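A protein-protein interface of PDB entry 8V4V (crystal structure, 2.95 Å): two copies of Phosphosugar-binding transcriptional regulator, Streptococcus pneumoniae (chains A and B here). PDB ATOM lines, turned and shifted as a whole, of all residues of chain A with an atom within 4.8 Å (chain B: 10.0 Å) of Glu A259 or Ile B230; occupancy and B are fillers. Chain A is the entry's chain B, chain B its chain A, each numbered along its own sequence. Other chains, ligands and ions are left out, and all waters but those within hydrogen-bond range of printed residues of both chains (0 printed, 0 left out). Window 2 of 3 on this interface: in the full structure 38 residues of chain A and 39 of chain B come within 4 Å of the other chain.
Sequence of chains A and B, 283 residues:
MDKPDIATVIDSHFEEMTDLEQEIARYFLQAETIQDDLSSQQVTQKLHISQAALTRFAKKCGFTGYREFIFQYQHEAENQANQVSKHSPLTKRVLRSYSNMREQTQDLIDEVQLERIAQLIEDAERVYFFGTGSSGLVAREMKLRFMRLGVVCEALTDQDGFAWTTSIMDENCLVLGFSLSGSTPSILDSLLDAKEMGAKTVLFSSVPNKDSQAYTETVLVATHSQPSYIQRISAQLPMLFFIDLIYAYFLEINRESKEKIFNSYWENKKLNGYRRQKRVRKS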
ATOM      1  N   LEU A 149      -3.576 -12.729  19.579  1.00  0.00           N
ATOM      2  CA  LEU A 149      -2.280 -12.447  18.982  1.00  0.00           C
ATOM      3  C   LEU A 149      -1.261 -12.002  20.022  1.00  0.00           C
ATOM      4  O   LEU A 149      -0.162 -11.568  19.658  1.00  0.00           O
ATOM      5  CB  LEU A 149      -2.420 -11.389  17.890  1.00  0.00           C
ATOM      6  CG  LEU A 149      -3.260 -11.820  16.690  1.00  0.00           C
ATOM      7  CD1 LEU A 149      -3.270 -10.721  15.635  1.00  0.00           C
ATOM      8  CD2 LEU A 149      -2.762 -13.128  16.095  1.00  0.00           C
ATOM      9  N   TYR A 247      -6.201  -5.257  11.896  1.00  0.00           N
ATOM     10  CA  TYR A 247      -5.791  -6.595  12.307  1.00  0.00           C
ATOM     11  C   TYR A 247      -4.889  -7.232  11.257  1.00  0.00           C
ATOM     12  O   TYR A 247      -3.868  -7.842  11.596  1.00  0.00           O
ATOM     13  CB  TYR A 247      -7.034  -7.451  12.567  1.00  0.00           C
ATOM     14  CG  TYR A 247      -6.769  -8.897  12.934  1.00  0.00           C
ATOM     15  CD1 TYR A 247      -6.650  -9.869  11.951  1.00  0.00           C
ATOM     16  CD2 TYR A 247      -6.659  -9.293  14.265  1.00  0.00           C
ATOM     17  CE1 TYR A 247      -6.418 -11.188  12.276  1.00  0.00           C
ATOM     18  CE2 TYR A 247      -6.425 -10.614  14.601  1.00  0.00           C
ATOM     19  CZ  TYR A 247      -6.307 -11.555  13.601  1.00  0.00           C
ATOM     20  OH  TYR A 247      -6.075 -12.869  13.925  1.00  0.00           O
ATOM     21  N   LEU A 251      -1.291  -8.198  12.168  1.00  0.00           N
ATOM     22  CA  LEU A 251      -0.932  -9.609  12.209  1.00  0.00           C
ATOM     23  C   LEU A 251       0.412  -9.866  11.543  1.00  0.00           C
ATOM     24  O   LEU A 251       1.127 -10.795  11.935  1.00  0.00           O
ATOM     25  CB  LEU A 251      -2.012 -10.452  11.535  1.00  0.00           C
ATOM     26  CG  LEU A 251      -1.680 -11.942  11.441  1.00  0.00           C
ATOM     27  CD1 LEU A 251      -1.747 -12.582  12.820  1.00  0.00           C
ATOM     28  CD2 LEU A 251      -2.611 -12.654  10.471  1.00  0.00           C
ATOM     29  N   ARG A 255       4.879 -11.943  12.821  1.00  0.00           N
ATOM     30  CA  ARG A 255       3.796 -12.909  12.689  1.00  0.00           C
ATOM     31  C   ARG A 255       4.135 -14.234  13.363  1.00  0.00           C
ATOM     32  O   ARG A 255       3.284 -14.817  14.045  1.00  0.00           O
ATOM     33  CB  ARG A 255       3.457 -13.145  11.220  1.00  0.00           C
ATOM     34  CG  ARG A 255       2.207 -13.984  11.082  1.00  0.00           C
ATOM     35  CD  ARG A 255       1.751 -14.210   9.653  1.00  0.00           C
ATOM     36  NE  ARG A 255       0.747 -15.268   9.638  1.00  0.00           N
ATOM     37  CZ  ARG A 255      -0.346 -15.272   8.888  1.00  0.00           C
ATOM     38  NH1 ARG A 255      -0.604 -14.294   8.033  1.00  0.00           N
ATOM     39  NH2 ARG A 255      -1.211 -16.275   9.007  1.00  0.00           N
ATOM     40  N   GLU A 256       5.364 -14.731  13.178  1.00  0.00           N
ATOM     41  CA  GLU A 256       5.729 -16.017  13.769  1.00  0.00           C
ATOM     42  C   GLU A 256       5.386 -16.043  15.250  1.00  0.00           C
ATOM     43  O   GLU A 256       4.819 -17.022  15.748  1.00  0.00           O
ATOM     44  CB  GLU A 256       7.222 -16.301  13.582  1.00  0.00           C
ATOM     45  CG  GLU A 256       7.611 -17.772  13.778  1.00  0.00           C
ATOM     46  CD  GLU A 256       7.959 -18.131  15.215  1.00  0.00           C
ATOM     47  OE1 GLU A 256       8.014 -17.221  16.073  1.00  0.00           O
ATOM     48  OE2 GLU A 256       8.190 -19.332  15.479  1.00  0.00           O
ATOM     49  N   SER A 257       5.718 -14.969  15.969  1.00  0.00           N
ATOM     50  CA  SER A 257       5.367 -14.890  17.383  1.00  0.00           C
ATOM     51  C   SER A 257       3.856 -14.956  17.572  1.00  0.00           C
ATOM     52  O   SER A 257       3.354 -15.791  18.330  1.00  0.00           O
ATOM     53  CB  SER A 257       5.944 -13.609  17.993  1.00  0.00           C
ATOM     54  OG  SER A 257       5.000 -12.553  17.982  1.00  0.00           O
ATOM     55  N   LYS A 258       3.109 -14.113  16.854  1.00  0.00           N
ATOM     56  CA  LYS A 258       1.672 -14.005  17.093  1.00  0.00           C
ATOM     57  C   LYS A 258       0.947 -15.302  16.752  1.00  0.00           C
ATOM     58  O   LYS A 258       0.122 -15.788  17.537  1.00  0.00           O
ATOM     59  CB  LYS A 258       1.107 -12.827  16.293  1.00  0.00           C
ATOM     60  CG  LYS A 258       1.728 -11.492  16.702  1.00  0.00           C
ATOM     61  CD  LYS A 258       1.262 -10.303  15.870  1.00  0.00           C
ATOM     62  CE  LYS A 258       1.792  -9.005  16.486  1.00  0.00           C
ATOM     63  NZ  LYS A 258       1.802  -7.846  15.555  1.00  0.00           N
ATOM     64  N   GLU A 259       1.253 -15.890  15.591  1.00  0.00           N
ATOM     65  CA  GLU A 259       0.591 -17.129  15.193  1.00  0.00           C
ATOM     66  C   GLU A 259       0.820 -18.229  16.224  1.00  0.00           C
ATOM     67  O   GLU A 259      -0.064 -19.059  16.465  1.00  0.00           O
ATOM     68  CB  GLU A 259       1.091 -17.566  13.816  1.00  0.00           C
ATOM     69  CG  GLU A 259       0.305 -18.699  13.170  1.00  0.00           C
ATOM     70  CD  GLU A 259       0.239 -18.572  11.656  1.00  0.00           C
ATOM     71  OE1 GLU A 259       1.028 -17.791  11.075  1.00  0.00           O
ATOM     72  OE2 GLU A 259      -0.594 -19.271  11.043  1.00  0.00           O
ATOM     73  N   LYS A 260       2.007 -18.256  16.836  1.00  0.00           N
ATOM     74  CA  LYS A 260       2.273 -19.234  17.886  1.00  0.00           C
ATOM     75  C   LYS A 260       1.360 -19.014  19.085  1.00  0.00           C
ATOM     76  O   LYS A 260       0.828 -19.973  19.655  1.00  0.00           O
ATOM     77  CB  LYS A 260       3.740 -19.153  18.310  1.00  0.00           C
ATOM     78  CG  LYS A 260       4.464 -20.492  18.358  1.00  0.00           C
ATOM     79  CD  LYS A 260       5.975 -20.309  18.228  1.00  0.00           C
ATOM     80  CE  LYS A 260       6.590 -19.790  19.521  1.00  0.00           C
ATOM     81  NZ  LYS A 260       8.015 -20.202  19.677  1.00  0.00           N
ATOM     82  N   ILE A 261       1.175 -17.755  19.488  1.00  0.00           N
ATOM     83  CA  ILE A 261       0.279 -17.453  20.600  1.00  0.00           C
ATOM     84  C   ILE A 261      -1.167 -17.743  20.217  1.00  0.00           C
ATOM     85  O   ILE A 261      -1.966 -18.171  21.057  1.00  0.00           O
ATOM     86  CB  ILE A 261       0.458 -15.989  21.040  1.00  0.00           C
ATOM     87  CG1 ILE A 261       1.936 -15.588  20.978  1.00  0.00           C
ATOM     88  CG2 ILE A 261      -0.095 -15.780  22.442  1.00  0.00           C
ATOM     89  CD1 ILE A 261       2.259 -14.300  21.702  1.00  0.00           C
ATOM     90  N   PHE A 262      -1.535 -17.495  18.960  1.00  0.00           N
ATOM     91  CA  PHE A 262      -2.895 -17.778  18.514  1.00  0.00           C
ATOM     92  C   PHE A 262      -3.177 -19.276  18.498  1.00  0.00           C
ATOM     93  O   PHE A 262      -4.262 -19.714  18.896  1.00  0.00           O
ATOM     94  CB  PHE A 262      -3.112 -17.181  17.125  1.00  0.00           C
ATOM     95  CG  PHE A 262      -4.495 -17.385  16.584  1.00  0.00           C
ATOM     96  CD1 PHE A 262      -5.564 -16.661  17.092  1.00  0.00           C
ATOM     97  CD2 PHE A 262      -4.728 -18.299  15.565  1.00  0.00           C
ATOM     98  CE1 PHE A 262      -6.847 -16.839  16.596  1.00  0.00           C
ATOM     99  CE2 PHE A 262      -6.010 -18.487  15.060  1.00  0.00           C
ATOM    100  CZ  PHE A 262      -7.072 -17.753  15.580  1.00  0.00           C
ATOM    101  N   ASN A 263      -2.223 -20.076  18.029  1.00  0.00           N
ATOM    102  CA  ASN A 263      -2.402 -21.521  17.991  1.00  0.00           C
ATOM    103  C   ASN A 263      -2.278 -22.177  19.358  1.00  0.00           C
ATOM    104  O   ASN A 263      -2.646 -23.348  19.498  1.00  0.00           O
ATOM    105  CB  ASN A 263      -1.382 -22.145  17.041  1.00  0.00           C
ATOM    106  CG  ASN A 263      -1.547 -21.667  15.613  1.00  0.00           C
ATOM    107  OD1 ASN A 263      -2.667 -21.479  15.136  1.00  0.00           O
ATOM    108  ND2 ASN A 263      -0.432 -21.496  14.913  1.00  0.00           N
ATOM    109  N   ARG B  93      -6.933  -8.011   0.225  1.00  0.00           N
ATOM    110  CA  ARG B  93      -7.417  -9.292   0.740  1.00  0.00           C
ATOM    111  C   ARG B  93      -8.611  -9.100   1.669  1.00  0.00           C
ATOM    112  O   ARG B  93      -9.603  -9.829   1.570  1.00  0.00           O
ATOM    113  CB  ARG B  93      -6.281 -10.031   1.464  1.00  0.00           C
ATOM    114  CG  ARG B  93      -6.696 -11.363   2.062  1.00  0.00           C
ATOM    115  CD  ARG B  93      -5.554 -12.007   2.823  1.00  0.00           C
ATOM    116  NE  ARG B  93      -5.577 -11.676   4.242  1.00  0.00           N
ATOM    117  CZ  ARG B  93      -4.501 -11.438   4.980  1.00  0.00           C
ATOM    118  NH1 ARG B  93      -3.286 -11.464   4.459  1.00  0.00           N
ATOM    119  NH2 ARG B  93      -4.650 -11.166   6.273  1.00  0.00           N
ATOM    120  N   VAL B  94      -8.540  -8.121   2.572  1.00  0.00           N
ATOM    121  CA  VAL B  94      -9.640  -7.902   3.509  1.00  0.00           C
ATOM    122  C   VAL B  94     -10.907  -7.505   2.760  1.00  0.00           C
ATOM    123  O   VAL B  94     -11.974  -8.106   2.940  1.00  0.00           O
ATOM    124  CB  VAL B  94      -9.248  -6.834   4.547  1.00  0.00           C
ATOM    125  CG1 VAL B  94     -10.491  -6.187   5.129  1.00  0.00           C
ATOM    126  CG2 VAL B  94      -8.382  -7.444   5.637  1.00  0.00           C
ATOM    127  N   HIS B 224     -16.515 -18.149   5.706  1.00  0.00           N
ATOM    128  CA  HIS B 224     -15.404 -17.256   5.415  1.00  0.00           C
ATOM    129  C   HIS B 224     -14.594 -17.790   4.241  1.00  0.00           C
ATOM    130  O   HIS B 224     -14.525 -18.998   4.003  1.00  0.00           O
ATOM    131  CB  HIS B 224     -14.505 -17.103   6.638  1.00  0.00           C
ATOM    132  CG  HIS B 224     -15.127 -16.324   7.755  1.00  0.00           C
ATOM    133  ND1 HIS B 224     -16.353 -16.645   8.299  1.00  0.00           N
ATOM    134  CD2 HIS B 224     -14.692 -15.233   8.427  1.00  0.00           C
ATOM    135  CE1 HIS B 224     -16.642 -15.788   9.262  1.00  0.00           C
ATOM    136  NE2 HIS B 224     -15.651 -14.920   9.359  1.00  0.00           N
ATOM    137  N   GLN B 226     -11.306 -17.183   3.819  1.00  0.00           N
ATOM    138  CA  GLN B 226      -9.906 -17.361   4.176  1.00  0.00           C
ATOM    139  C   GLN B 226      -9.702 -18.771   4.700  1.00  0.00           C
ATOM    140  O   GLN B 226     -10.370 -19.154   5.673  1.00  0.00           O
ATOM    141  CB  GLN B 226      -9.483 -16.343   5.229  1.00  0.00           C
ATOM    142  CG  GLN B 226      -9.119 -14.986   4.652  1.00  0.00           C
ATOM    143  CD  GLN B 226      -7.912 -15.051   3.740  1.00  0.00           C
ATOM    144  OE1 GLN B 226      -6.873 -15.596   4.110  1.00  0.00           O
ATOM    145  NE2 GLN B 226      -8.052 -14.517   2.531  1.00  0.00           N
ATOM    146  N   PRO B 227      -8.812 -19.575   4.114  1.00  0.00           N
ATOM    147  CA  PRO B 227      -8.667 -20.953   4.619  1.00  0.00           C
ATOM    148  C   PRO B 227      -8.328 -20.998   6.099  1.00  0.00           C
ATOM    149  O   PRO B 227      -8.964 -21.739   6.862  1.00  0.00           O
ATOM    150  CB  PRO B 227      -7.544 -21.542   3.750  1.00  0.00           C
ATOM    151  CG  PRO B 227      -7.252 -20.544   2.679  1.00  0.00           C
ATOM    152  CD  PRO B 227      -7.788 -19.222   3.114  1.00  0.00           C
ATOM    153  N   SER B 228      -7.366 -20.185   6.532  1.00  0.00           N
ATOM    154  CA  SER B 228      -6.840 -20.246   7.887  1.00  0.00           C
ATOM    155  C   SER B 228      -7.650 -19.364   8.825  1.00  0.00           C
ATOM    156  O   SER B 228      -8.037 -18.247   8.469  1.00  0.00           O
ATOM    157  CB  SER B 228      -5.375 -19.813   7.905  1.00  0.00           C
ATOM    158  OG  SER B 228      -5.242 -18.483   7.440  1.00  0.00           O
ATOM    159  N   TYR B 229      -7.889 -19.878  10.034  1.00  0.00           N
ATOM    160  CA  TYR B 229      -8.667 -19.140  11.023  1.00  0.00           C
ATOM    161  C   TYR B 229      -8.065 -17.762  11.276  1.00  0.00           C
ATOM    162  O   TYR B 229      -8.774 -16.750  11.285  1.00  0.00           O
ATOM    163  CB  TYR B 229      -8.725 -19.920  12.338  1.00  0.00           C
ATOM    164  CG  TYR B 229      -9.444 -21.245  12.281  1.00  0.00           C
ATOM    165  CD1 TYR B 229     -10.782 -21.315  11.940  1.00  0.00           C
ATOM    166  CD2 TYR B 229      -8.781 -22.431  12.581  1.00  0.00           C
ATOM    167  CE1 TYR B 229     -11.443 -22.526  11.894  1.00  0.00           C
ATOM    168  CE2 TYR B 229      -9.435 -23.651  12.536  1.00  0.00           C
ATOM    169  CZ  TYR B 229     -10.767 -23.693  12.191  1.00  0.00           C
ATOM    170  OH  TYR B 229     -11.427 -24.901  12.143  1.00  0.00           O
ATOM    171  N   ILE B 230      -6.745 -17.706  11.471  1.00  0.00           N
ATOM    172  CA  ILE B 230      -6.103 -16.489  11.961  1.00  0.00           C
ATOM    173  C   ILE B 230      -6.247 -15.339  10.975  1.00  0.00           C
ATOM    174  O   ILE B 230      -6.321 -14.170  11.379  1.00  0.00           O
ATOM    175  CB  ILE B 230      -4.622 -16.782  12.271  1.00  0.00           C
ATOM    176  CG1 ILE B 230      -4.011 -15.672  13.124  1.00  0.00           C
ATOM    177  CG2 ILE B 230      -3.831 -16.949  10.980  1.00  0.00           C
ATOM    178  CD1 ILE B 230      -2.637 -16.017  13.662  1.00  0.00           C
ATOM    179  N   GLN B 231      -6.280 -15.634   9.680  1.00  0.00           N
ATOM    180  CA  GLN B 231      -6.340 -14.603   8.652  1.00  0.00           C
ATOM    181  C   GLN B 231      -7.762 -14.215   8.272  1.00  0.00           C
ATOM    182  O   GLN B 231      -7.943 -13.392   7.368  1.00  0.00           O
ATOM    183  CB  GLN B 231      -5.594 -15.077   7.407  1.00  0.00           C
ATOM    184  CG  GLN B 231      -4.157 -14.612   7.337  1.00  0.00           C
ATOM    185  CD  GLN B 231      -3.487 -15.002   6.036  1.00  0.00           C
ATOM    186  OE1 GLN B 231      -2.288 -15.275   6.001  1.00  0.00           O
ATOM    187  NE2 GLN B 231      -4.260 -15.027   4.955  1.00  0.00           N
ATOM    188  N   ARG B 232      -8.761 -14.781   8.935  1.00  0.00           N
ATOM    189  CA  ARG B 232     -10.151 -14.556   8.577  1.00  0.00           C
ATOM    190  C   ARG B 232     -10.629 -13.196   9.077  1.00  0.00           C
ATOM    191  O   ARG B 232     -10.106 -12.648  10.052  1.00  0.00           O
ATOM    192  CB  ARG B 232     -11.017 -15.671   9.163  1.00  0.00           C
ATOM    193  CG  ARG B 232     -10.635 -17.085   8.707  1.00  0.00           C
ATOM    194  CD  ARG B 232     -11.887 -17.725   8.157  1.00  0.00           C
ATOM    195  NE  ARG B 232     -11.938 -19.181   8.167  1.00  0.00           N
ATOM    196  CZ  ARG B 232     -12.815 -19.889   8.866  1.00  0.00           C
ATOM    197  NH1 ARG B 232     -13.511 -19.347   9.851  1.00  0.00           N
ATOM    198  NH2 ARG B 232     -12.995 -21.174   8.573  1.00  0.00           N
ATOM    199  N   ILE B 233     -11.626 -12.643   8.385  1.00  0.00           N
ATOM    200  CA  ILE B 233     -12.256 -11.398   8.815  1.00  0.00           C
ATOM    201  C   ILE B 233     -13.202 -11.725   9.962  1.00  0.00           C
ATOM    202  O   ILE B 233     -13.401 -12.899  10.298  1.00  0.00           O
ATOM    203  CB  ILE B 233     -12.997 -10.696   7.663  1.00  0.00           C
ATOM    204  CG1 ILE B 233     -14.110 -11.583   7.102  1.00  0.00           C
ATOM    205  CG2 ILE B 233     -12.017 -10.301   6.563  1.00  0.00           C
ATOM    206  CD1 ILE B 233     -14.915 -10.900   6.000  1.00  0.00           C
ATOM    207  N   SER B 234     -13.805 -10.692  10.554  1.00  0.00           N
ATOM    208  CA  SER B 234     -14.617 -10.862  11.755  1.00  0.00           C
ATOM    209  C   SER B 234     -15.561 -12.048  11.619  1.00  0.00           C
ATOM    210  O   SER B 234     -16.194 -12.241  10.578  1.00  0.00           O
ATOM    211  CB  SER B 234     -15.424  -9.590  12.028  1.00  0.00           C
ATOM    212  OG  SER B 234     -16.638  -9.885  12.695  1.00  0.00           O
ATOM    213  N   ALA B 235     -15.646 -12.845  12.688  1.00  0.00           N
ATOM    214  CA  ALA B 235     -16.491 -14.033  12.698  1.00  0.00           C
ATOM    215  C   ALA B 235     -17.971 -13.699  12.806  1.00  0.00           C
ATOM    216  O   ALA B 235     -18.806 -14.583  12.591  1.00  0.00           O
ATOM    217  CB  ALA B 235     -16.084 -14.957  13.851  1.00  0.00           C
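The backbone carbonyl oxygen (O) of Ile B230 is in hydrogen-bond range of the side-chain hydroxyl (OH) of Tyr A247.
NH1 of Arg A255 lies within hydrogen-bond range of OE1 of Gln B231 (2.8 Å).
The guanidinium group of Arg A255 lies within salt-bridge range of the side-chain carboxylate of Glu A259, 2.9 Å away.
The backbone carbonyl oxygen of Glu A259 lies within hydrogen-bond range of the side-chain amide nitrogen of Asn A263 (2.9 Å).
OE1 of Gln B226 lies within hydrogen-bond range of NE2 of Gln B231 (2.8 Å).
Among the printed residues, pairs that only touch across the chains: Leu A149 with Ile B230, Leu A251 with Ile B230, Arg A255 with Ile B230, Glu A259 with Ile B230 and Phe A262 with Ile B230.
Glu A259 touches one residue of chain B.
Ile B230 touches just these residues of chain A: Leu A149, Tyr A247, Leu A251, Arg A255, Glu A259 and Phe A262.
Ser A257 touches none of the printed residues of chain B.
No residue of chain B comes within 4 Å of Asn A263.
Of the printed residues of chain B, Tyr A247 touches Ile B230 (2.9 Å).
Of the printed residues of chain B, Leu A149 touches Ile B230 (3.8 Å).
Of the printed residues of chain B, Leu A251 touches Ile B230 (3.6 Å).
Of the printed residues of chain B, Arg A255 touches Ile B230 and Gln B231.
Of the printed residues of chain A, Gln B231 touches Arg A255 (2.8 Å).
Gln B226 touches none of the printed residues of chain A.
The nearest residue of chain B that does not touch Glu A259 is Ser B228 (5.7 Å).
The nearest printed residue of chain A that does not touch Ile B230 is Lys A258 (4.8 Å).
The nearest printed residue of chain A that does not touch Gln B231 is Leu A251 (4.01 Å).
Of the 13 printed residues of chain B, 2 touch a printed residue of chain A.
Printed residues of chain B that touch a printed residue of chain A: Ile B230 and Gln B231.
Hydrophobic or aromatic side chains of chain B that line the printed part of chain A: Ile B230.
Hydrophobic or aromatic side chains of chain A that line the printed part of chain B: Leu A149, Tyr A247, Leu A251 and Phe A262.
Among the printed residues, 7 pairs touch across the chains.
Among the printed residues, no Asp or Glu carboxylate lies within 4 Å of a Lys or Arg side-chain nitrogen of the other chain.
No position is printed for both chains.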
